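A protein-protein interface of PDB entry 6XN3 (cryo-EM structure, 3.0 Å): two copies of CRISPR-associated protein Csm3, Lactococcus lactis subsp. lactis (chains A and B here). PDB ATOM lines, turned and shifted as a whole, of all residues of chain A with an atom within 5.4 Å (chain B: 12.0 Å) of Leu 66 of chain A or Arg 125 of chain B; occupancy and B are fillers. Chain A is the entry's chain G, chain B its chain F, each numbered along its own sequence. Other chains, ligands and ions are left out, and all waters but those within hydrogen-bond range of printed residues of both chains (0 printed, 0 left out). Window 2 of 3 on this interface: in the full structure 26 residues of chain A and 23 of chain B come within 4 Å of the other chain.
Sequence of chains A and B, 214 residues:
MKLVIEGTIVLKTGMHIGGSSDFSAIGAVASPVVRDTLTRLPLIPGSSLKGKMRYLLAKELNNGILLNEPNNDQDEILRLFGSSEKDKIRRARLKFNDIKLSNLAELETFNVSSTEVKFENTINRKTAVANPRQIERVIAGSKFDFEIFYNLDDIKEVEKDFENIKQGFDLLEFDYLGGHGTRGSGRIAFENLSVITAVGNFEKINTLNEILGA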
ATOM      1  N   ARG A  54      -0.187 -11.219 -11.884  1.00  0.00           N
ATOM      2  CA  ARG A  54       0.768 -10.300 -11.286  1.00  0.00           C
ATOM      3  C   ARG A  54       0.358  -9.932  -9.872  1.00  0.00           C
ATOM      4  O   ARG A  54       1.207  -9.877  -8.979  1.00  0.00           O
ATOM      5  CB  ARG A  54       0.920  -9.046 -12.142  1.00  0.00           C
ATOM      6  CG  ARG A  54       1.923  -8.064 -11.577  1.00  0.00           C
ATOM      7  CD  ARG A  54       2.291  -6.989 -12.553  1.00  0.00           C
ATOM      8  NE  ARG A  54       3.291  -6.101 -11.986  1.00  0.00           N
ATOM      9  CZ  ARG A  54       4.078  -5.320 -12.709  1.00  0.00           C
ATOM     10  NH1 ARG A  54       3.981  -5.328 -14.024  1.00  0.00           N
ATOM     11  NH2 ARG A  54       4.965  -4.541 -12.120  1.00  0.00           N
ATOM     12  N   TYR A  55      -0.944  -9.749  -9.638  1.00  0.00           N
ATOM     13  CA  TYR A  55      -1.415  -9.406  -8.300  1.00  0.00           C
ATOM     14  C   TYR A  55      -1.168 -10.535  -7.312  1.00  0.00           C
ATOM     15  O   TYR A  55      -0.605 -10.317  -6.233  1.00  0.00           O
ATOM     16  CB  TYR A  55      -2.897  -9.067  -8.327  1.00  0.00           C
ATOM     17  CG  TYR A  55      -3.416  -8.713  -6.964  1.00  0.00           C
ATOM     18  CD1 TYR A  55      -3.015  -7.544  -6.345  1.00  0.00           C
ATOM     19  CD2 TYR A  55      -4.295  -9.545  -6.293  1.00  0.00           C
ATOM     20  CE1 TYR A  55      -3.475  -7.206  -5.107  1.00  0.00           C
ATOM     21  CE2 TYR A  55      -4.761  -9.213  -5.047  1.00  0.00           C
ATOM     22  CZ  TYR A  55      -4.343  -8.040  -4.461  1.00  0.00           C
ATOM     23  OH  TYR A  55      -4.797  -7.691  -3.216  1.00  0.00           O
ATOM     24  N   ALA A  58       2.682 -11.279  -6.930  1.00  0.00           N
ATOM     25  CA  ALA A  58       3.358 -10.255  -6.160  1.00  0.00           C
ATOM     26  C   ALA A  58       2.780 -10.123  -4.768  1.00  0.00           C
ATOM     27  O   ALA A  58       3.292  -9.332  -3.979  1.00  0.00           O
ATOM     28  CB  ALA A  58       3.284  -8.921  -6.888  1.00  0.00           C
ATOM     29  N   LYS A  59       1.693 -10.830  -4.464  1.00  0.00           N
ATOM     30  CA  LYS A  59       1.274 -10.915  -3.073  1.00  0.00           C
ATOM     31  C   LYS A  59       1.983 -12.059  -2.356  1.00  0.00           C
ATOM     32  O   LYS A  59       2.274 -11.958  -1.161  1.00  0.00           O
ATOM     33  CB  LYS A  59      -0.243 -11.076  -2.987  1.00  0.00           C
ATOM     34  CG  LYS A  59      -0.802 -10.949  -1.586  1.00  0.00           C
ATOM     35  CD  LYS A  59      -2.246 -11.386  -1.508  1.00  0.00           C
ATOM     36  CE  LYS A  59      -3.167 -10.308  -1.994  1.00  0.00           C
ATOM     37  NZ  LYS A  59      -3.185  -9.162  -1.059  1.00  0.00           N
ATOM     38  N   ASN A  62       6.978 -10.748  -1.515  1.00  0.00           N
ATOM     39  CA  ASN A  62       6.762  -9.659  -0.552  1.00  0.00           C
ATOM     40  C   ASN A  62       5.751 -10.115   0.503  1.00  0.00           C
ATOM     41  O   ASN A  62       4.642  -9.592   0.613  1.00  0.00           O
ATOM     42  CB  ASN A  62       6.320  -8.357  -1.250  1.00  0.00           C
ATOM     43  CG  ASN A  62       6.296  -7.160  -0.327  1.00  0.00           C
ATOM     44  OD1 ASN A  62       6.761  -7.214   0.808  1.00  0.00           O
ATOM     45  ND2 ASN A  62       5.734  -6.066  -0.813  1.00  0.00           N
ATOM     46  N   GLY A  64       2.999 -11.839   2.517  1.00  0.00           N
ATOM     47  CA  GLY A  64       1.913 -11.221   3.238  1.00  0.00           C
ATOM     48  C   GLY A  64       1.167 -10.222   2.383  1.00  0.00           C
ATOM     49  O   GLY A  64       0.412 -10.587   1.480  1.00  0.00           O
ATOM     50  N   ILE A  65       1.390  -8.947   2.676  1.00  0.00           N
ATOM     51  CA  ILE A  65       0.601  -7.868   2.134  1.00  0.00           C
ATOM     52  C   ILE A  65       1.261  -7.308   0.878  1.00  0.00           C
ATOM     53  O   ILE A  65       2.463  -7.438   0.667  1.00  0.00           O
ATOM     54  CB  ILE A  65       0.383  -6.765   3.189  1.00  0.00           C
ATOM     55  CG1 ILE A  65       1.717  -6.129   3.579  1.00  0.00           C
ATOM     56  CG2 ILE A  65      -0.297  -7.340   4.414  1.00  0.00           C
ATOM     57  N   LEU A  66       0.448  -6.681   0.017  1.00  0.00           N
ATOM     58  CA  LEU A  66       0.917  -5.968  -1.176  1.00  0.00           C
ATOM     59  C   LEU A  66       0.258  -4.590  -1.201  1.00  0.00           C
ATOM     60  O   LEU A  66      -0.766  -4.380  -1.852  1.00  0.00           O
ATOM     61  CB  LEU A  66       0.602  -6.763  -2.420  1.00  0.00           C
ATOM     62  CG  LEU A  66       1.155  -6.255  -3.743  1.00  0.00           C
ATOM     63  CD1 LEU A  66       2.649  -6.131  -3.671  1.00  0.00           C
ATOM     64  CD2 LEU A  66       0.742  -7.185  -4.846  1.00  0.00           C
ATOM     65  N   LEU A  67       0.828  -3.655  -0.452  1.00  0.00           N
ATOM     66  CA  LEU A  67       0.324  -2.287  -0.402  1.00  0.00           C
ATOM     67  C   LEU A  67       1.255  -1.336  -1.156  1.00  0.00           C
ATOM     68  O   LEU A  67       1.838  -0.425  -0.573  1.00  0.00           O
ATOM     69  CB  LEU A  67       0.151  -1.846   1.048  1.00  0.00           C
ATOM     70  CG  LEU A  67      -1.090  -2.189   1.882  1.00  0.00           C
ATOM     71  CD1 LEU A  67      -2.326  -1.551   1.301  1.00  0.00           C
ATOM     72  CD2 LEU A  67      -1.312  -3.671   2.080  1.00  0.00           C
ATOM     73  N   ASN A  68       1.388  -1.531  -2.468  1.00  0.00           N
ATOM     74  CA  ASN A  68       2.278  -0.637  -3.202  1.00  0.00           C
ATOM     75  C   ASN A  68       1.843  -0.496  -4.652  1.00  0.00           C
ATOM     76  O   ASN A  68       1.031  -1.270  -5.158  1.00  0.00           O
ATOM     77  CB  ASN A  68       3.736  -1.103  -3.135  1.00  0.00           C
ATOM     78  CG  ASN A  68       3.914  -2.539  -3.553  1.00  0.00           C
ATOM     79  OD1 ASN A  68       3.681  -2.903  -4.700  1.00  0.00           O
ATOM     80  ND2 ASN A  68       4.342  -3.367  -2.617  1.00  0.00           N
ATOM     81  N   GLU A  69       2.421   0.510  -5.306  1.00  0.00           N
ATOM     82  CA  GLU A  69       2.221   0.773  -6.720  1.00  0.00           C
ATOM     83  C   GLU A  69       2.789  -0.371  -7.559  1.00  0.00           C
ATOM     84  O   GLU A  69       3.788  -0.983  -7.182  1.00  0.00           O
ATOM     85  CB  GLU A  69       2.894   2.097  -7.079  1.00  0.00           C
ATOM     86  CG  GLU A  69       2.690   3.177  -6.042  1.00  0.00           C
ATOM     87  CD  GLU A  69       1.288   3.744  -6.075  1.00  0.00           C
ATOM     88  OE1 GLU A  69       0.726   4.002  -4.990  1.00  0.00           O
ATOM     89  OE2 GLU A  69       0.750   3.936  -7.185  1.00  0.00           O
ATOM     90  N   PRO A  70       2.173  -0.685  -8.705  1.00  0.00           N
ATOM     91  CA  PRO A  70       2.614  -1.870  -9.454  1.00  0.00           C
ATOM     92  C   PRO A  70       3.895  -1.680 -10.226  1.00  0.00           C
ATOM     93  O   PRO A  70       4.389  -2.646 -10.816  1.00  0.00           O
ATOM     94  CB  PRO A  70       1.435  -2.151 -10.389  1.00  0.00           C
ATOM     95  CG  PRO A  70       0.748  -0.850 -10.558  1.00  0.00           C
ATOM     96  CD  PRO A  70       1.241   0.118  -9.516  1.00  0.00           C
ATOM     97  N   ASP A  73       7.349  -3.359  -7.141  1.00  0.00           N
ATOM     98  CA  ASP A  73       7.032  -4.204  -5.998  1.00  0.00           C
ATOM     99  C   ASP A  73       8.138  -5.182  -5.643  1.00  0.00           C
ATOM    100  O   ASP A  73       8.647  -5.129  -4.523  1.00  0.00           O
ATOM    101  CB  ASP A  73       5.703  -4.947  -6.233  1.00  0.00           C
ATOM    102  CG  ASP A  73       5.597  -5.543  -7.609  1.00  0.00           C
ATOM    103  OD1 ASP A  73       6.577  -5.483  -8.352  1.00  0.00           O
ATOM    104  OD2 ASP A  73       4.511  -6.031  -7.966  1.00  0.00           O
ATOM    105  N   GLU B 120     -11.184  -1.935 -20.327  1.00  0.00           N
ATOM    106  CA  GLU B 120     -10.088  -2.401 -19.504  1.00  0.00           C
ATOM    107  C   GLU B 120      -9.919  -1.429 -18.342  1.00  0.00           C
ATOM    108  O   GLU B 120     -10.298  -0.266 -18.446  1.00  0.00           O
ATOM    109  CB  GLU B 120      -8.827  -2.518 -20.371  1.00  0.00           C
ATOM    110  CG  GLU B 120      -7.604  -3.053 -19.698  1.00  0.00           C
ATOM    111  CD  GLU B 120      -7.768  -4.490 -19.281  1.00  0.00           C
ATOM    112  OE1 GLU B 120      -8.573  -5.185 -19.925  1.00  0.00           O
ATOM    113  OE2 GLU B 120      -7.115  -4.925 -18.316  1.00  0.00           O
ATOM    114  N   ASN B 121      -9.392  -1.917 -17.215  1.00  0.00           N
ATOM    115  CA  ASN B 121      -9.024  -1.033 -16.116  1.00  0.00           C
ATOM    116  C   ASN B 121      -7.715  -1.476 -15.484  1.00  0.00           C
ATOM    117  O   ASN B 121      -7.186  -2.546 -15.783  1.00  0.00           O
ATOM    118  CB  ASN B 121     -10.076  -0.956 -15.008  1.00  0.00           C
ATOM    119  CG  ASN B 121     -10.529  -2.300 -14.517  1.00  0.00           C
ATOM    120  OD1 ASN B 121      -9.791  -3.042 -13.873  1.00  0.00           O
ATOM    121  ND2 ASN B 121     -11.798  -2.562 -14.705  1.00  0.00           N
ATOM    122  N   THR B 122      -7.209  -0.629 -14.591  1.00  0.00           N
ATOM    123  CA  THR B 122      -6.211  -1.010 -13.606  1.00  0.00           C
ATOM    124  C   THR B 122      -6.840  -0.895 -12.234  1.00  0.00           C
ATOM    125  O   THR B 122      -7.869  -0.241 -12.065  1.00  0.00           O
ATOM    126  CB  THR B 122      -4.965  -0.135 -13.628  1.00  0.00           C
ATOM    127  OG1 THR B 122      -4.027  -0.636 -12.670  1.00  0.00           O
ATOM    128  CG2 THR B 122      -5.284   1.290 -13.267  1.00  0.00           C
ATOM    129  N   ILE B 123      -6.240  -1.563 -11.260  1.00  0.00           N
ATOM    130  CA  ILE B 123      -6.682  -1.483  -9.877  1.00  0.00           C
ATOM    131  C   ILE B 123      -5.493  -1.077  -9.029  1.00  0.00           C
ATOM    132  O   ILE B 123      -4.445  -1.732  -9.068  1.00  0.00           O
ATOM    133  CB  ILE B 123      -7.279  -2.813  -9.392  1.00  0.00           C
ATOM    134  CG1 ILE B 123      -8.520  -3.156 -10.197  1.00  0.00           C
ATOM    135  CG2 ILE B 123      -7.661  -2.717  -7.940  1.00  0.00           C
ATOM    136  CD1 ILE B 123      -9.004  -4.535  -9.963  1.00  0.00           C
ATOM    137  N   ASN B 124      -5.643   0.024  -8.300  1.00  0.00           N
ATOM    138  CA  ASN B 124      -4.636   0.436  -7.337  1.00  0.00           C
ATOM    139  C   ASN B 124      -4.564  -0.616  -6.248  1.00  0.00           C
ATOM    140  O   ASN B 124      -5.591  -1.140  -5.821  1.00  0.00           O
ATOM    141  CB  ASN B 124      -4.991   1.795  -6.752  1.00  0.00           C
ATOM    142  CG  ASN B 124      -3.824   2.449  -6.054  1.00  0.00           C
ATOM    143  OD1 ASN B 124      -2.704   1.947  -6.090  1.00  0.00           O
ATOM    144  ND2 ASN B 124      -4.080   3.581  -5.413  1.00  0.00           N
ATOM    145  N   ARG B 125      -3.359  -0.972  -5.832  1.00  0.00           N
ATOM    146  CA  ARG B 125      -3.256  -2.072  -4.892  1.00  0.00           C
ATOM    147  C   ARG B 125      -3.509  -1.635  -3.463  1.00  0.00           C
ATOM    148  O   ARG B 125      -3.905  -2.464  -2.641  1.00  0.00           O
ATOM    149  CB  ARG B 125      -1.897  -2.732  -5.029  1.00  0.00           C
ATOM    150  CG  ARG B 125      -1.720  -3.350  -6.383  1.00  0.00           C
ATOM    151  CD  ARG B 125      -0.393  -4.007  -6.521  1.00  0.00           C
ATOM    152  NE  ARG B 125      -0.267  -4.627  -7.827  1.00  0.00           N
ATOM    153  CZ  ARG B 125       0.887  -4.976  -8.368  1.00  0.00           C
ATOM    154  NH1 ARG B 125       2.017  -4.758  -7.713  1.00  0.00           N
ATOM    155  NH2 ARG B 125       0.910  -5.536  -9.565  1.00  0.00           N
ATOM    156  N   LYS B 126      -3.305  -0.362  -3.148  1.00  0.00           N
ATOM    157  CA  LYS B 126      -3.590   0.096  -1.800  1.00  0.00           C
ATOM    158  C   LYS B 126      -5.048   0.492  -1.639  1.00  0.00           C
ATOM    159  O   LYS B 126      -5.715   0.043  -0.703  1.00  0.00           O
ATOM    160  CB  LYS B 126      -2.686   1.271  -1.428  1.00  0.00           C
ATOM    161  CG  LYS B 126      -2.983   1.834  -0.050  1.00  0.00           C
ATOM    162  CD  LYS B 126      -1.922   2.812   0.402  1.00  0.00           C
ATOM    163  CE  LYS B 126      -2.058   4.135  -0.322  1.00  0.00           C
ATOM    164  NZ  LYS B 126      -3.284   4.860   0.091  1.00  0.00           N
ATOM    165  N   THR B 127      -5.558   1.318  -2.538  1.00  0.00           N
ATOM    166  CA  THR B 127      -6.897   1.860  -2.384  1.00  0.00           C
ATOM    167  C   THR B 127      -7.972   1.036  -3.070  1.00  0.00           C
ATOM    168  O   THR B 127      -9.142   1.391  -2.951  1.00  0.00           O
ATOM    169  CB  THR B 127      -6.955   3.290  -2.917  1.00  0.00           C
ATOM    170  OG1 THR B 127      -6.636   3.292  -4.312  1.00  0.00           O
ATOM    171  CG2 THR B 127      -5.974   4.171  -2.170  1.00  0.00           C
ATOM    172  N   ALA B 128      -7.600  -0.003  -3.826  1.00  0.00           N
ATOM    173  CA  ALA B 128      -8.508  -0.997  -4.423  1.00  0.00           C
ATOM    174  C   ALA B 128      -9.588  -0.388  -5.322  1.00  0.00           C
ATOM    175  O   ALA B 128     -10.637  -0.998  -5.536  1.00  0.00           O
ATOM    176  CB  ALA B 128      -9.147  -1.875  -3.345  1.00  0.00           C
ATOM    177  N   VAL B 129      -9.357   0.802  -5.861  1.00  0.00           N
ATOM    178  CA  VAL B 129     -10.311   1.480  -6.727  1.00  0.00           C
ATOM    179  C   VAL B 129      -9.900   1.226  -8.165  1.00  0.00           C
ATOM    180  O   VAL B 129      -8.733   1.417  -8.522  1.00  0.00           O
ATOM    181  CB  VAL B 129     -10.356   2.987  -6.427  1.00  0.00           C
ATOM    182  CG1 VAL B 129     -11.224   3.714  -7.428  1.00  0.00           C
ATOM    183  CG2 VAL B 129     -10.872   3.235  -5.033  1.00  0.00           C
ATOM    184  N   ALA B 130     -10.846   0.792  -8.990  1.00  0.00           N
ATOM    185  CA  ALA B 130     -10.559   0.544 -10.391  1.00  0.00           C
ATOM    186  C   ALA B 130     -10.395   1.859 -11.140  1.00  0.00           C
ATOM    187  O   ALA B 130     -10.676   2.940 -10.626  1.00  0.00           O
ATOM    188  CB  ALA B 130     -11.656  -0.298 -11.025  1.00  0.00           C
ATOM    189  N   ASN B 131      -9.930   1.768 -12.383  1.00  0.00           N
ATOM    190  CA  ASN B 131      -9.651   2.953 -13.187  1.00  0.00           C
ATOM    191  C   ASN B 131      -9.813   2.569 -14.638  1.00  0.00           C
ATOM    192  O   ASN B 131      -8.859   2.129 -15.289  1.00  0.00           O
ATOM    193  CB  ASN B 131      -8.249   3.492 -12.917  1.00  0.00           C
ATOM    194  CG  ASN B 131      -8.024   4.842 -13.522  1.00  0.00           C
ATOM    195  OD1 ASN B 131      -8.959   5.607 -13.718  1.00  0.00           O
ATOM    196  ND2 ASN B 131      -6.775   5.148 -13.830  1.00  0.00           N
ATOM    197  N   ARG B 133     -10.499   2.179 -18.734  1.00  0.00           N
ATOM    198  CA  ARG B 133     -10.066   2.797 -19.974  1.00  0.00           C
ATOM    199  C   ARG B 133     -10.703   2.047 -21.126  1.00  0.00           C
ATOM    200  O   ARG B 133     -10.973   0.849 -21.020  1.00  0.00           O
ATOM    201  CB  ARG B 133      -8.547   2.776 -20.107  1.00  0.00           C
ATOM    202  CG  ARG B 133      -7.935   1.410 -19.983  1.00  0.00           C
ATOM    203  CD  ARG B 133      -6.475   1.464 -20.333  1.00  0.00           C
ATOM    204  NE  ARG B 133      -5.803   0.179 -20.218  1.00  0.00           N
ATOM    205  CZ  ARG B 133      -5.404  -0.350 -19.070  1.00  0.00           C
ATOM    206  NH1 ARG B 133      -5.618   0.283 -17.932  1.00  0.00           N
ATOM    207  NH2 ARG B 133      -4.780  -1.513 -19.056  1.00  0.00           N
ATOM    208  N   ARG B 183      -0.074  -7.286 -22.834  1.00  0.00           N
ATOM    209  CA  ARG B 183      -1.385  -7.635 -22.318  1.00  0.00           C
ATOM    210  C   ARG B 183      -2.283  -8.266 -23.367  1.00  0.00           C
ATOM    211  O   ARG B 183      -3.488  -8.005 -23.367  1.00  0.00           O
ATOM    212  CB  ARG B 183      -2.099  -6.425 -21.738  1.00  0.00           C
ATOM    213  CG  ARG B 183      -1.675  -6.021 -20.373  1.00  0.00           C
ATOM    214  CD  ARG B 183      -0.468  -5.133 -20.370  1.00  0.00           C
ATOM    215  NE  ARG B 183      -0.700  -3.973 -21.215  1.00  0.00           N
ATOM    216  CZ  ARG B 183      -1.376  -2.899 -20.835  1.00  0.00           C
ATOM    217  NH1 ARG B 183      -1.954  -2.876 -19.655  1.00  0.00           N
ATOM    218  NH2 ARG B 183      -1.536  -1.877 -21.657  1.00  0.00           N
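The side-chain carboxylate (OD2) of Asp 73 of chain A is in salt-bridge range of the guanidinium group (NH1) of Arg 125 of chain B, 2.8 Å away. NE of Arg 54 of chain A sits close to NH2 of Arg 125 of chain B, 3.4 Å away.
Among the printed residues, pairs that only touch across the chains: Asn 68 of chain A with Arg 125 of chain B, Pro 70 of chain A with Arg 125 of chain B, Leu 67 of chain A with Lys 126 of chain B and Leu 66 of chain A with Arg 125 of chain B.
Leu 66 of chain A touches just one residue of chain B: Arg 125. Arg 125 of chain B touches just these residues of chain A: Arg 54 (3.4 Å), Leu 66 (3.8 Å), Asn 68 (3.3 Å), Pro 70 (3.4 Å) and Asp 73 (2.8 Å). Arg 54 of chain A touches just one residue of chain B: Arg 125 (3.4 Å). No residue of chain B comes within 4 Å of Tyr 55 of chain A. No residue of chain B comes within 4 Å of Ala 58 of chain A. No residue of chain B comes within 4 Å of Gly 64 of chain A. Ile 65 of chain A touches none of the printed residues of chain B. Of chain B, only Lys 126 (3.7 Å) comes within 4 Å of Leu 67 of chain A. Asn 68 of chain A touches just one residue of chain B: Arg 125. No residue of chain B comes within 4 Å of Glu 69 of chain A. Pro 70 of chain A touches just one residue of chain B: Arg 125 (3.4 Å). Asp 73 of chain A touches one residue of chain B. Of the printed residues of chain A, Lys 126 of chain B touches Leu 67. The nearest residue of chain B that does not touch Leu 66 of chain A is Lys 126 of chain B (4.9 Å).
Along chain A the printed residues that touch a printed residue of chain B span positions 54 to 73. Of the 14 printed residues of chain B, 2 touch a printed residue of chain A. Along chain B the printed residues that touch a printed residue of chain A span positions 125 to 126. Among the printed residues, 6 pairs touch across the chains. Among the printed residues, Asp or Glu carboxylates within 4 Å of a Lys or Arg side-chain nitrogen of the other chain: Asp 73 of chain A with Arg 125 of chain B.
No position is printed for both chains.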
